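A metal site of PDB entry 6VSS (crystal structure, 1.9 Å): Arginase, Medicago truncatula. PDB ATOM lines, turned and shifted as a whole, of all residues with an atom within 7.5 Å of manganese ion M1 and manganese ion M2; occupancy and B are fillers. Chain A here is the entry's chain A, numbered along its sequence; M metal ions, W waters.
The side-chain carboxylate (OD2) of Asp 184 lies close to a ring nitrogen (NE2) of His 182. The side-chain carboxylate of Glu 312 lies within hydrogen-bond range of the backbone NH of His 160, 2.9 Å away. NE2 of His 160 lies within hydrogen-bond range of OG of Ser 267 (2.7 Å). The side-chain hydroxyl (OG) of Ser 163 lies close to a ring nitrogen (NE2) of His 160 (3.3 Å). The backbone carbonyl oxygen (O) of Asp 269 is in hydrogen-bond range of the side-chain hydroxyl (OG) of Ser 272 (2.9 Å). The backbone carbonyl oxygen (O) of Asp 188 is in hydrogen-bond range of the backbone NH (N) of Phe 204. The side-chain carboxylate (OD1) of Asp 271 lies close to the backbone NH (N) of Ala 185, at 3.4 Å. The side-chain carboxylate of Glu 285 is in hydrogen-bond range of a ring nitrogen (NE2) of His 186 (3.0 Å).
Of the 26 residues printed, 4 come within 4 Å of manganese ion M1. The nearest printed residue that does not touch manganese ion M1 is His 200 (4.4 Å).
Four residues have an atom within 4 Å of manganese ion M2: Asp 184, His 186, Asp 269 and Asp 271. The nearest printed residue that does not touch manganese ion M2 is Ala 185 (4.3 Å).
Manganese ion M1 is bound by OD2 of Asp 184. Water W2 binds manganese ion M1, 2.1 Å away. ND1 of His 160 is bound to manganese ion M1 (2.2 Å). Manganese ion M1 is bound by OD2 of Asp 269. Manganese ion M1 is bound by OD2 of Asp 188 (2.2 Å).
Water W2 binds manganese ion M2. OD2 of Asp 269 is bound to manganese ion M2 (2.2 Å). Manganese ion M2 is bound by OD1 of Asp 184, at 2.2 Å. OD1 of Asp 271 binds manganese ion M2 (2.2 Å). The side-chain carboxylate (OD2) of Asp 271 is bound to manganese ion M2. Manganese ion M2 is bound by ND1 of His 186 (2.3 Å). Water W1 binds manganese ion M2. Manganese ion M2 has seven donor atoms within binding distance.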
ATOM      1  N   ASP A 159       8.540 -25.022 -11.720  1.00  0.00           N
ATOM      2  CA  ASP A 159       7.885 -24.059 -10.797  1.00  0.00           C
ATOM      3  C   ASP A 159       6.753 -23.344 -11.563  1.00  0.00           C
ATOM      4  O   ASP A 159       6.658 -23.482 -12.834  1.00  0.00           O
ATOM      5  CB  ASP A 159       8.908 -23.213 -10.018  1.00  0.00           C
ATOM      6  CG  ASP A 159       9.568 -22.086 -10.817  1.00  0.00           C
ATOM      7  OD1 ASP A 159       8.859 -21.521 -11.666  1.00  0.00           O
ATOM      8  OD2 ASP A 159      10.804 -21.838 -10.605  1.00  0.00           O
ATOM      9  N   HIS A 160       5.892 -22.679 -10.826  1.00  0.00           N
ATOM     10  CA  HIS A 160       4.650 -22.047 -11.370  1.00  0.00           C
ATOM     11  C   HIS A 160       4.964 -20.903 -12.333  1.00  0.00           C
ATOM     12  O   HIS A 160       4.024 -20.445 -13.033  1.00  0.00           O
ATOM     13  CB  HIS A 160       3.728 -21.654 -10.184  1.00  0.00           C
ATOM     14  CG  HIS A 160       2.295 -21.889 -10.518  1.00  0.00           C
ATOM     15  ND1 HIS A 160       1.388 -22.192  -9.591  1.00  0.00           N
ATOM     16  CD2 HIS A 160       1.690 -21.960 -11.736  1.00  0.00           C
ATOM     17  CE1 HIS A 160       0.224 -22.441 -10.179  1.00  0.00           C
ATOM     18  NE2 HIS A 160       0.386 -22.303 -11.528  1.00  0.00           N
ATOM     19  N   SER A 161       6.189 -20.402 -12.388  1.00  0.00           N
ATOM     20  CA  SER A 161       6.541 -19.302 -13.323  1.00  0.00           C
ATOM     21  C   SER A 161       6.227 -19.765 -14.740  1.00  0.00           C
ATOM     22  O   SER A 161       5.891 -18.901 -15.562  1.00  0.00           O
ATOM     23  CB  SER A 161       7.967 -18.893 -13.260  1.00  0.00           C
ATOM     24  OG  SER A 161       8.825 -19.900 -13.850  1.00  0.00           O
ATOM     25  N   SER A 163       3.591 -21.203 -16.028  1.00  0.00           N
ATOM     26  CA  SER A 163       2.179 -20.991 -16.470  1.00  0.00           C
ATOM     27  C   SER A 163       2.045 -19.749 -17.399  1.00  0.00           C
ATOM     28  O   SER A 163       1.223 -19.747 -18.338  1.00  0.00           O
ATOM     29  CB  SER A 163       1.282 -20.872 -15.306  1.00  0.00           C
ATOM     30  OG  SER A 163       1.164 -22.160 -14.726  1.00  0.00           O
ATOM     31  N   HIS A 182      -7.526 -22.598 -11.364  1.00  0.00           N
ATOM     32  CA  HIS A 182      -6.185 -22.485 -10.782  1.00  0.00           C
ATOM     33  C   HIS A 182      -6.304 -22.992  -9.368  1.00  0.00           C
ATOM     34  O   HIS A 182      -6.966 -22.331  -8.512  1.00  0.00           O
ATOM     35  CB  HIS A 182      -5.707 -21.028 -10.912  1.00  0.00           C
ATOM     36  CG  HIS A 182      -4.433 -20.652 -10.243  1.00  0.00           C
ATOM     37  ND1 HIS A 182      -4.197 -19.364  -9.790  1.00  0.00           N
ATOM     38  CD2 HIS A 182      -3.338 -21.379  -9.909  1.00  0.00           C
ATOM     39  CE1 HIS A 182      -3.029 -19.336  -9.210  1.00  0.00           C
ATOM     40  NE2 HIS A 182      -2.464 -20.552  -9.281  1.00  0.00           N
ATOM     41  N   PHE A 183      -5.668 -24.112  -9.118  1.00  0.00           N
ATOM     42  CA  PHE A 183      -5.537 -24.577  -7.735  1.00  0.00           C
ATOM     43  C   PHE A 183      -4.168 -24.165  -7.243  1.00  0.00           C
ATOM     44  O   PHE A 183      -3.184 -24.472  -7.915  1.00  0.00           O
ATOM     45  CB  PHE A 183      -5.652 -26.098  -7.636  1.00  0.00           C
ATOM     46  CG  PHE A 183      -6.901 -26.678  -8.213  1.00  0.00           C
ATOM     47  CD1 PHE A 183      -6.980 -26.979  -9.575  1.00  0.00           C
ATOM     48  CD2 PHE A 183      -7.976 -26.977  -7.413  1.00  0.00           C
ATOM     49  CE1 PHE A 183      -8.101 -27.598 -10.098  1.00  0.00           C
ATOM     50  CE2 PHE A 183      -9.120 -27.555  -7.931  1.00  0.00           C
ATOM     51  CZ  PHE A 183      -9.182 -27.867  -9.278  1.00  0.00           C
ATOM     52  N   ASP A 184      -4.132 -23.565  -6.069  1.00  0.00           N
ATOM     53  CA  ASP A 184      -2.876 -23.153  -5.436  1.00  0.00           C
ATOM     54  C   ASP A 184      -3.149 -22.792  -3.977  1.00  0.00           C
ATOM     55  O   ASP A 184      -4.234 -22.349  -3.707  1.00  0.00           O
ATOM     56  CB  ASP A 184      -2.385 -21.856  -6.081  1.00  0.00           C
ATOM     57  CG  ASP A 184      -0.888 -21.729  -6.161  1.00  0.00           C
ATOM     58  OD1 ASP A 184      -0.242 -21.794  -5.095  1.00  0.00           O
ATOM     59  OD2 ASP A 184      -0.432 -21.576  -7.286  1.00  0.00           O
ATOM     60  N   ALA A 185      -2.163 -22.851  -3.115  1.00  0.00           N
ATOM     61  CA  ALA A 185      -2.176 -22.224  -1.763  1.00  0.00           C
ATOM     62  C   ALA A 185      -1.990 -20.695  -1.913  1.00  0.00           C
ATOM     63  O   ALA A 185      -2.237 -19.953  -0.932  1.00  0.00           O
ATOM     64  CB  ALA A 185      -1.052 -22.803  -0.948  1.00  0.00           C
ATOM     65  N   HIS A 186      -1.393 -20.273  -3.026  1.00  0.00           N
ATOM     66  CA  HIS A 186      -0.909 -18.871  -3.221  1.00  0.00           C
ATOM     67  C   HIS A 186      -1.556 -18.265  -4.461  1.00  0.00           C
ATOM     68  O   HIS A 186      -1.610 -18.875  -5.515  1.00  0.00           O
ATOM     69  CB  HIS A 186       0.637 -18.808  -3.392  1.00  0.00           C
ATOM     70  CG  HIS A 186       1.390 -19.685  -2.466  1.00  0.00           C
ATOM     71  ND1 HIS A 186       1.754 -21.043  -2.807  1.00  0.00           N
ATOM     72  CD2 HIS A 186       1.817 -19.410  -1.201  1.00  0.00           C
ATOM     73  CE1 HIS A 186       2.321 -21.551  -1.732  1.00  0.00           C
ATOM     74  NE2 HIS A 186       2.384 -20.554  -0.714  1.00  0.00           N
ATOM     75  N   PRO A 187      -1.994 -17.006  -4.418  1.00  0.00           N
ATOM     76  CA  PRO A 187      -2.573 -16.393  -5.614  1.00  0.00           C
ATOM     77  C   PRO A 187      -1.612 -16.228  -6.787  1.00  0.00           C
ATOM     78  O   PRO A 187      -2.092 -16.153  -7.921  1.00  0.00           O
ATOM     79  CB  PRO A 187      -3.099 -15.040  -5.154  1.00  0.00           C
ATOM     80  CG  PRO A 187      -3.129 -15.122  -3.626  1.00  0.00           C
ATOM     81  CD  PRO A 187      -2.022 -16.101  -3.258  1.00  0.00           C
ATOM     82  N   ASP A 188      -0.294 -16.095  -6.531  1.00  0.00           N
ATOM     83  CA  ASP A 188       0.675 -15.859  -7.643  1.00  0.00           C
ATOM     84  C   ASP A 188       0.248 -14.634  -8.499  1.00  0.00           C
ATOM     85  O   ASP A 188       0.400 -14.644  -9.777  1.00  0.00           O
ATOM     86  CB  ASP A 188       0.779 -17.119  -8.499  1.00  0.00           C
ATOM     87  CG  ASP A 188       1.407 -18.330  -7.805  1.00  0.00           C
ATOM     88  OD1 ASP A 188       1.865 -18.220  -6.587  1.00  0.00           O
ATOM     89  OD2 ASP A 188       1.435 -19.363  -8.488  1.00  0.00           O
ATOM     90  N   HIS A 200       7.945 -17.274  -9.760  1.00  0.00           N
ATOM     91  CA  HIS A 200       6.814 -18.253  -9.664  1.00  0.00           C
ATOM     92  C   HIS A 200       5.687 -17.680  -8.795  1.00  0.00           C
ATOM     93  O   HIS A 200       4.648 -18.317  -8.736  1.00  0.00           O
ATOM     94  CB  HIS A 200       7.286 -19.622  -9.148  1.00  0.00           C
ATOM     95  CG  HIS A 200       7.644 -19.681  -7.699  1.00  0.00           C
ATOM     96  ND1 HIS A 200       7.681 -20.895  -6.998  1.00  0.00           N
ATOM     97  CD2 HIS A 200       7.967 -18.711  -6.815  1.00  0.00           C
ATOM     98  CE1 HIS A 200       8.036 -20.673  -5.751  1.00  0.00           C
ATOM     99  NE2 HIS A 200       8.223 -19.330  -5.605  1.00  0.00           N
ATOM    100  N   ALA A 201       5.887 -16.527  -8.150  1.00  0.00           N
ATOM    101  CA  ALA A 201       4.828 -15.818  -7.407  1.00  0.00           C
ATOM    102  C   ALA A 201       4.160 -14.683  -8.236  1.00  0.00           C
ATOM    103  O   ALA A 201       3.325 -13.941  -7.640  1.00  0.00           O
ATOM    104  CB  ALA A 201       5.425 -15.283  -6.136  1.00  0.00           C
ATOM    105  N   PRO A 203       3.138 -15.308 -12.074  1.00  0.00           N
ATOM    106  CA  PRO A 203       2.675 -15.651 -13.413  1.00  0.00           C
ATOM    107  C   PRO A 203       1.235 -15.202 -13.716  1.00  0.00           C
ATOM    108  O   PRO A 203       0.979 -14.920 -14.865  1.00  0.00           O
ATOM    109  CB  PRO A 203       2.807 -17.182 -13.476  1.00  0.00           C
ATOM    110  CG  PRO A 203       2.634 -17.568 -12.001  1.00  0.00           C
ATOM    111  CD  PRO A 203       3.345 -16.491 -11.203  1.00  0.00           C
ATOM    112  N   PHE A 204       0.355 -15.110 -12.721  1.00  0.00           N
ATOM    113  CA  PHE A 204      -1.069 -14.772 -13.017  1.00  0.00           C
ATOM    114  C   PHE A 204      -1.182 -13.260 -13.200  1.00  0.00           C
ATOM    115  O   PHE A 204      -2.090 -12.847 -13.978  1.00  0.00           O
ATOM    116  CB  PHE A 204      -2.051 -15.492 -12.069  1.00  0.00           C
ATOM    117  CG  PHE A 204      -2.037 -16.984 -12.343  1.00  0.00           C
ATOM    118  CD1 PHE A 204      -2.809 -17.537 -13.344  1.00  0.00           C
ATOM    119  CD2 PHE A 204      -1.148 -17.832 -11.683  1.00  0.00           C
ATOM    120  CE1 PHE A 204      -2.774 -18.900 -13.639  1.00  0.00           C
ATOM    121  CE2 PHE A 204      -1.071 -19.178 -12.024  1.00  0.00           C
ATOM    122  CZ  PHE A 204      -1.862 -19.711 -13.012  1.00  0.00           C
ATOM    123  N   SER A 267      -4.663 -25.044 -14.306  1.00  0.00           N
ATOM    124  CA  SER A 267      -3.350 -25.005 -13.637  1.00  0.00           C
ATOM    125  C   SER A 267      -3.478 -25.601 -12.236  1.00  0.00           C
ATOM    126  O   SER A 267      -4.185 -25.040 -11.358  1.00  0.00           O
ATOM    127  CB  SER A 267      -2.769 -23.592 -13.618  1.00  0.00           C
ATOM    128  OG  SER A 267      -1.439 -23.554 -13.075  1.00  0.00           O
ATOM    129  N   ILE A 268      -2.703 -26.663 -11.996  1.00  0.00           N
ATOM    130  CA  ILE A 268      -2.703 -27.347 -10.695  1.00  0.00           C
ATOM    131  C   ILE A 268      -1.323 -27.179 -10.076  1.00  0.00           C
ATOM    132  O   ILE A 268      -0.335 -27.801 -10.609  1.00  0.00           O
ATOM    133  CB  ILE A 268      -3.108 -28.822 -10.894  1.00  0.00           C
ATOM    134  CG1 ILE A 268      -4.269 -28.968 -11.866  1.00  0.00           C
ATOM    135  CG2 ILE A 268      -3.335 -29.425  -9.528  1.00  0.00           C
ATOM    136  CD1 ILE A 268      -4.868 -30.373 -11.974  1.00  0.00           C
ATOM    137  N   ASP A 269      -1.260 -26.380  -9.001  1.00  0.00           N
ATOM    138  CA  ASP A 269      -0.077 -26.273  -8.098  1.00  0.00           C
ATOM    139  C   ASP A 269      -0.294 -27.311  -6.996  1.00  0.00           C
ATOM    140  O   ASP A 269      -1.229 -27.216  -6.270  1.00  0.00           O
ATOM    141  CB  ASP A 269       0.156 -24.810  -7.641  1.00  0.00           C
ATOM    142  CG  ASP A 269       1.380 -24.478  -6.749  1.00  0.00           C
ATOM    143  OD1 ASP A 269       1.947 -25.449  -6.130  1.00  0.00           O
ATOM    144  OD2 ASP A 269       1.772 -23.280  -6.679  1.00  0.00           O
ATOM    145  N   VAL A 270       0.573 -28.307  -6.943  1.00  0.00           N
ATOM    146  CA  VAL A 270       0.470 -29.433  -5.984  1.00  0.00           C
ATOM    147  C   VAL A 270       0.448 -28.841  -4.547  1.00  0.00           C
ATOM    148  O   VAL A 270      -0.173 -29.484  -3.698  1.00  0.00           O
ATOM    149  CB  VAL A 270       1.623 -30.402  -6.251  1.00  0.00           C
ATOM    150  CG1 VAL A 270       1.741 -31.487  -5.250  1.00  0.00           C
ATOM    151  CG2 VAL A 270       1.532 -30.976  -7.659  1.00  0.00           C
ATOM    152  N   ASP A 271       0.977 -27.647  -4.276  1.00  0.00           N
ATOM    153  CA  ASP A 271       0.984 -27.087  -2.879  1.00  0.00           C
ATOM    154  C   ASP A 271      -0.445 -26.577  -2.483  1.00  0.00           C
ATOM    155  O   ASP A 271      -0.713 -26.212  -1.280  1.00  0.00           O
ATOM    156  CB  ASP A 271       2.100 -26.063  -2.717  1.00  0.00           C
ATOM    157  CG  ASP A 271       1.967 -24.661  -3.318  1.00  0.00           C
ATOM    158  OD1 ASP A 271       0.878 -24.247  -3.673  1.00  0.00           O
ATOM    159  OD2 ASP A 271       2.983 -23.968  -3.420  1.00  0.00           O
ATOM    160  N   SER A 272      -1.365 -26.569  -3.451  1.00  0.00           N
ATOM    161  CA  SER A 272      -2.814 -26.444  -3.158  1.00  0.00           C
ATOM    162  C   SER A 272      -3.296 -27.532  -2.160  1.00  0.00           C
ATOM    163  O   SER A 272      -4.196 -27.262  -1.333  1.00  0.00           O
ATOM    164  CB  SER A 272      -3.604 -26.473  -4.465  1.00  0.00           C
ATOM    165  OG  SER A 272      -3.718 -27.819  -4.997  1.00  0.00           O
ATOM    166  N   VAL A 281       6.670 -30.582  -2.013  1.00  0.00           N
ATOM    167  CA  VAL A 281       6.578 -29.190  -2.546  1.00  0.00           C
ATOM    168  C   VAL A 281       7.559 -28.278  -1.803  1.00  0.00           C
ATOM    169  O   VAL A 281       8.041 -28.654  -0.725  1.00  0.00           O
ATOM    170  CB  VAL A 281       5.134 -28.630  -2.411  1.00  0.00           C
ATOM    171  CG1 VAL A 281       4.152 -29.476  -3.187  1.00  0.00           C
ATOM    172  CG2 VAL A 281       4.733 -28.551  -0.928  1.00  0.00           C
ATOM    173  N   HIS A 283       6.735 -25.117  -0.898  1.00  0.00           N
ATOM    174  CA  HIS A 283       6.014 -24.188   0.002  1.00  0.00           C
ATOM    175  C   HIS A 283       4.946 -24.929   0.782  1.00  0.00           C
ATOM    176  O   HIS A 283       3.825 -24.992   0.334  1.00  0.00           O
ATOM    177  CB  HIS A 283       5.453 -22.990  -0.747  1.00  0.00           C
ATOM    178  CG  HIS A 283       6.545 -22.116  -1.265  1.00  0.00           C
ATOM    179  ND1 HIS A 283       7.187 -21.162  -0.472  1.00  0.00           N
ATOM    180  CD2 HIS A 283       7.189 -22.133  -2.458  1.00  0.00           C
ATOM    181  CE1 HIS A 283       8.160 -20.605  -1.164  1.00  0.00           C
ATOM    182  NE2 HIS A 283       8.188 -21.189  -2.402  1.00  0.00           N
ATOM    183  N   GLU A 285       2.135 -25.158   3.210  1.00  0.00           N
ATOM    184  CA  GLU A 285       1.143 -24.269   3.831  1.00  0.00           C
ATOM    185  C   GLU A 285       0.064 -25.086   4.500  1.00  0.00           C
ATOM    186  O   GLU A 285      -0.858 -25.543   3.838  1.00  0.00           O
ATOM    187  CB  GLU A 285       0.574 -23.362   2.747  1.00  0.00           C
ATOM    188  CG  GLU A 285       1.623 -22.578   2.014  1.00  0.00           C
ATOM    189  CD  GLU A 285       2.090 -21.335   2.751  1.00  0.00           C
ATOM    190  OE1 GLU A 285       1.577 -21.072   3.911  1.00  0.00           O
ATOM    191  OE2 GLU A 285       2.966 -20.626   2.182  1.00  0.00           O
ATOM    192  N   VAL A 311       2.189 -28.414 -11.624  1.00  0.00           N
ATOM    193  CA  VAL A 311       3.433 -27.683 -11.290  1.00  0.00           C
ATOM    194  C   VAL A 311       3.698 -27.794  -9.776  1.00  0.00           C
ATOM    195  O   VAL A 311       2.791 -28.086  -8.980  1.00  0.00           O
ATOM    196  CB  VAL A 311       3.408 -26.198 -11.713  1.00  0.00           C
ATOM    197  CG1 VAL A 311       3.112 -26.028 -13.207  1.00  0.00           C
ATOM    198  CG2 VAL A 311       2.407 -25.413 -10.887  1.00  0.00           C
ATOM    199  N   GLU A 312       4.947 -27.476  -9.471  1.00  0.00           N
ATOM    200  CA  GLU A 312       5.518 -27.329  -8.111  1.00  0.00           C
ATOM    201  C   GLU A 312       5.693 -28.689  -7.447  1.00  0.00           C
ATOM    202  O   GLU A 312       5.956 -28.669  -6.232  1.00  0.00           O
ATOM    203  CB  GLU A 312       4.745 -26.335  -7.258  1.00  0.00           C
ATOM    204  CG  GLU A 312       4.810 -24.887  -7.790  1.00  0.00           C
ATOM    205  CD  GLU A 312       6.043 -24.080  -7.398  1.00  0.00           C
ATOM    206  OE1 GLU A 312       6.782 -24.528  -6.429  1.00  0.00           O
ATOM    207  OE2 GLU A 312       6.279 -23.016  -8.000  1.00  0.00           O
HETATM  208 MN    MN M   1       1.619 -21.344  -7.623  1.00  0.00          MN
HETATM  209 MN    MN M   2       1.822 -22.455  -4.629  1.00  0.00          MN
HETATM  210  O   HOH W   1       4.354 -21.752  -5.224  1.00  0.00           O
HETATM  211  O   HOH W   2       2.069 -20.553  -5.685  1.00  0.00           O
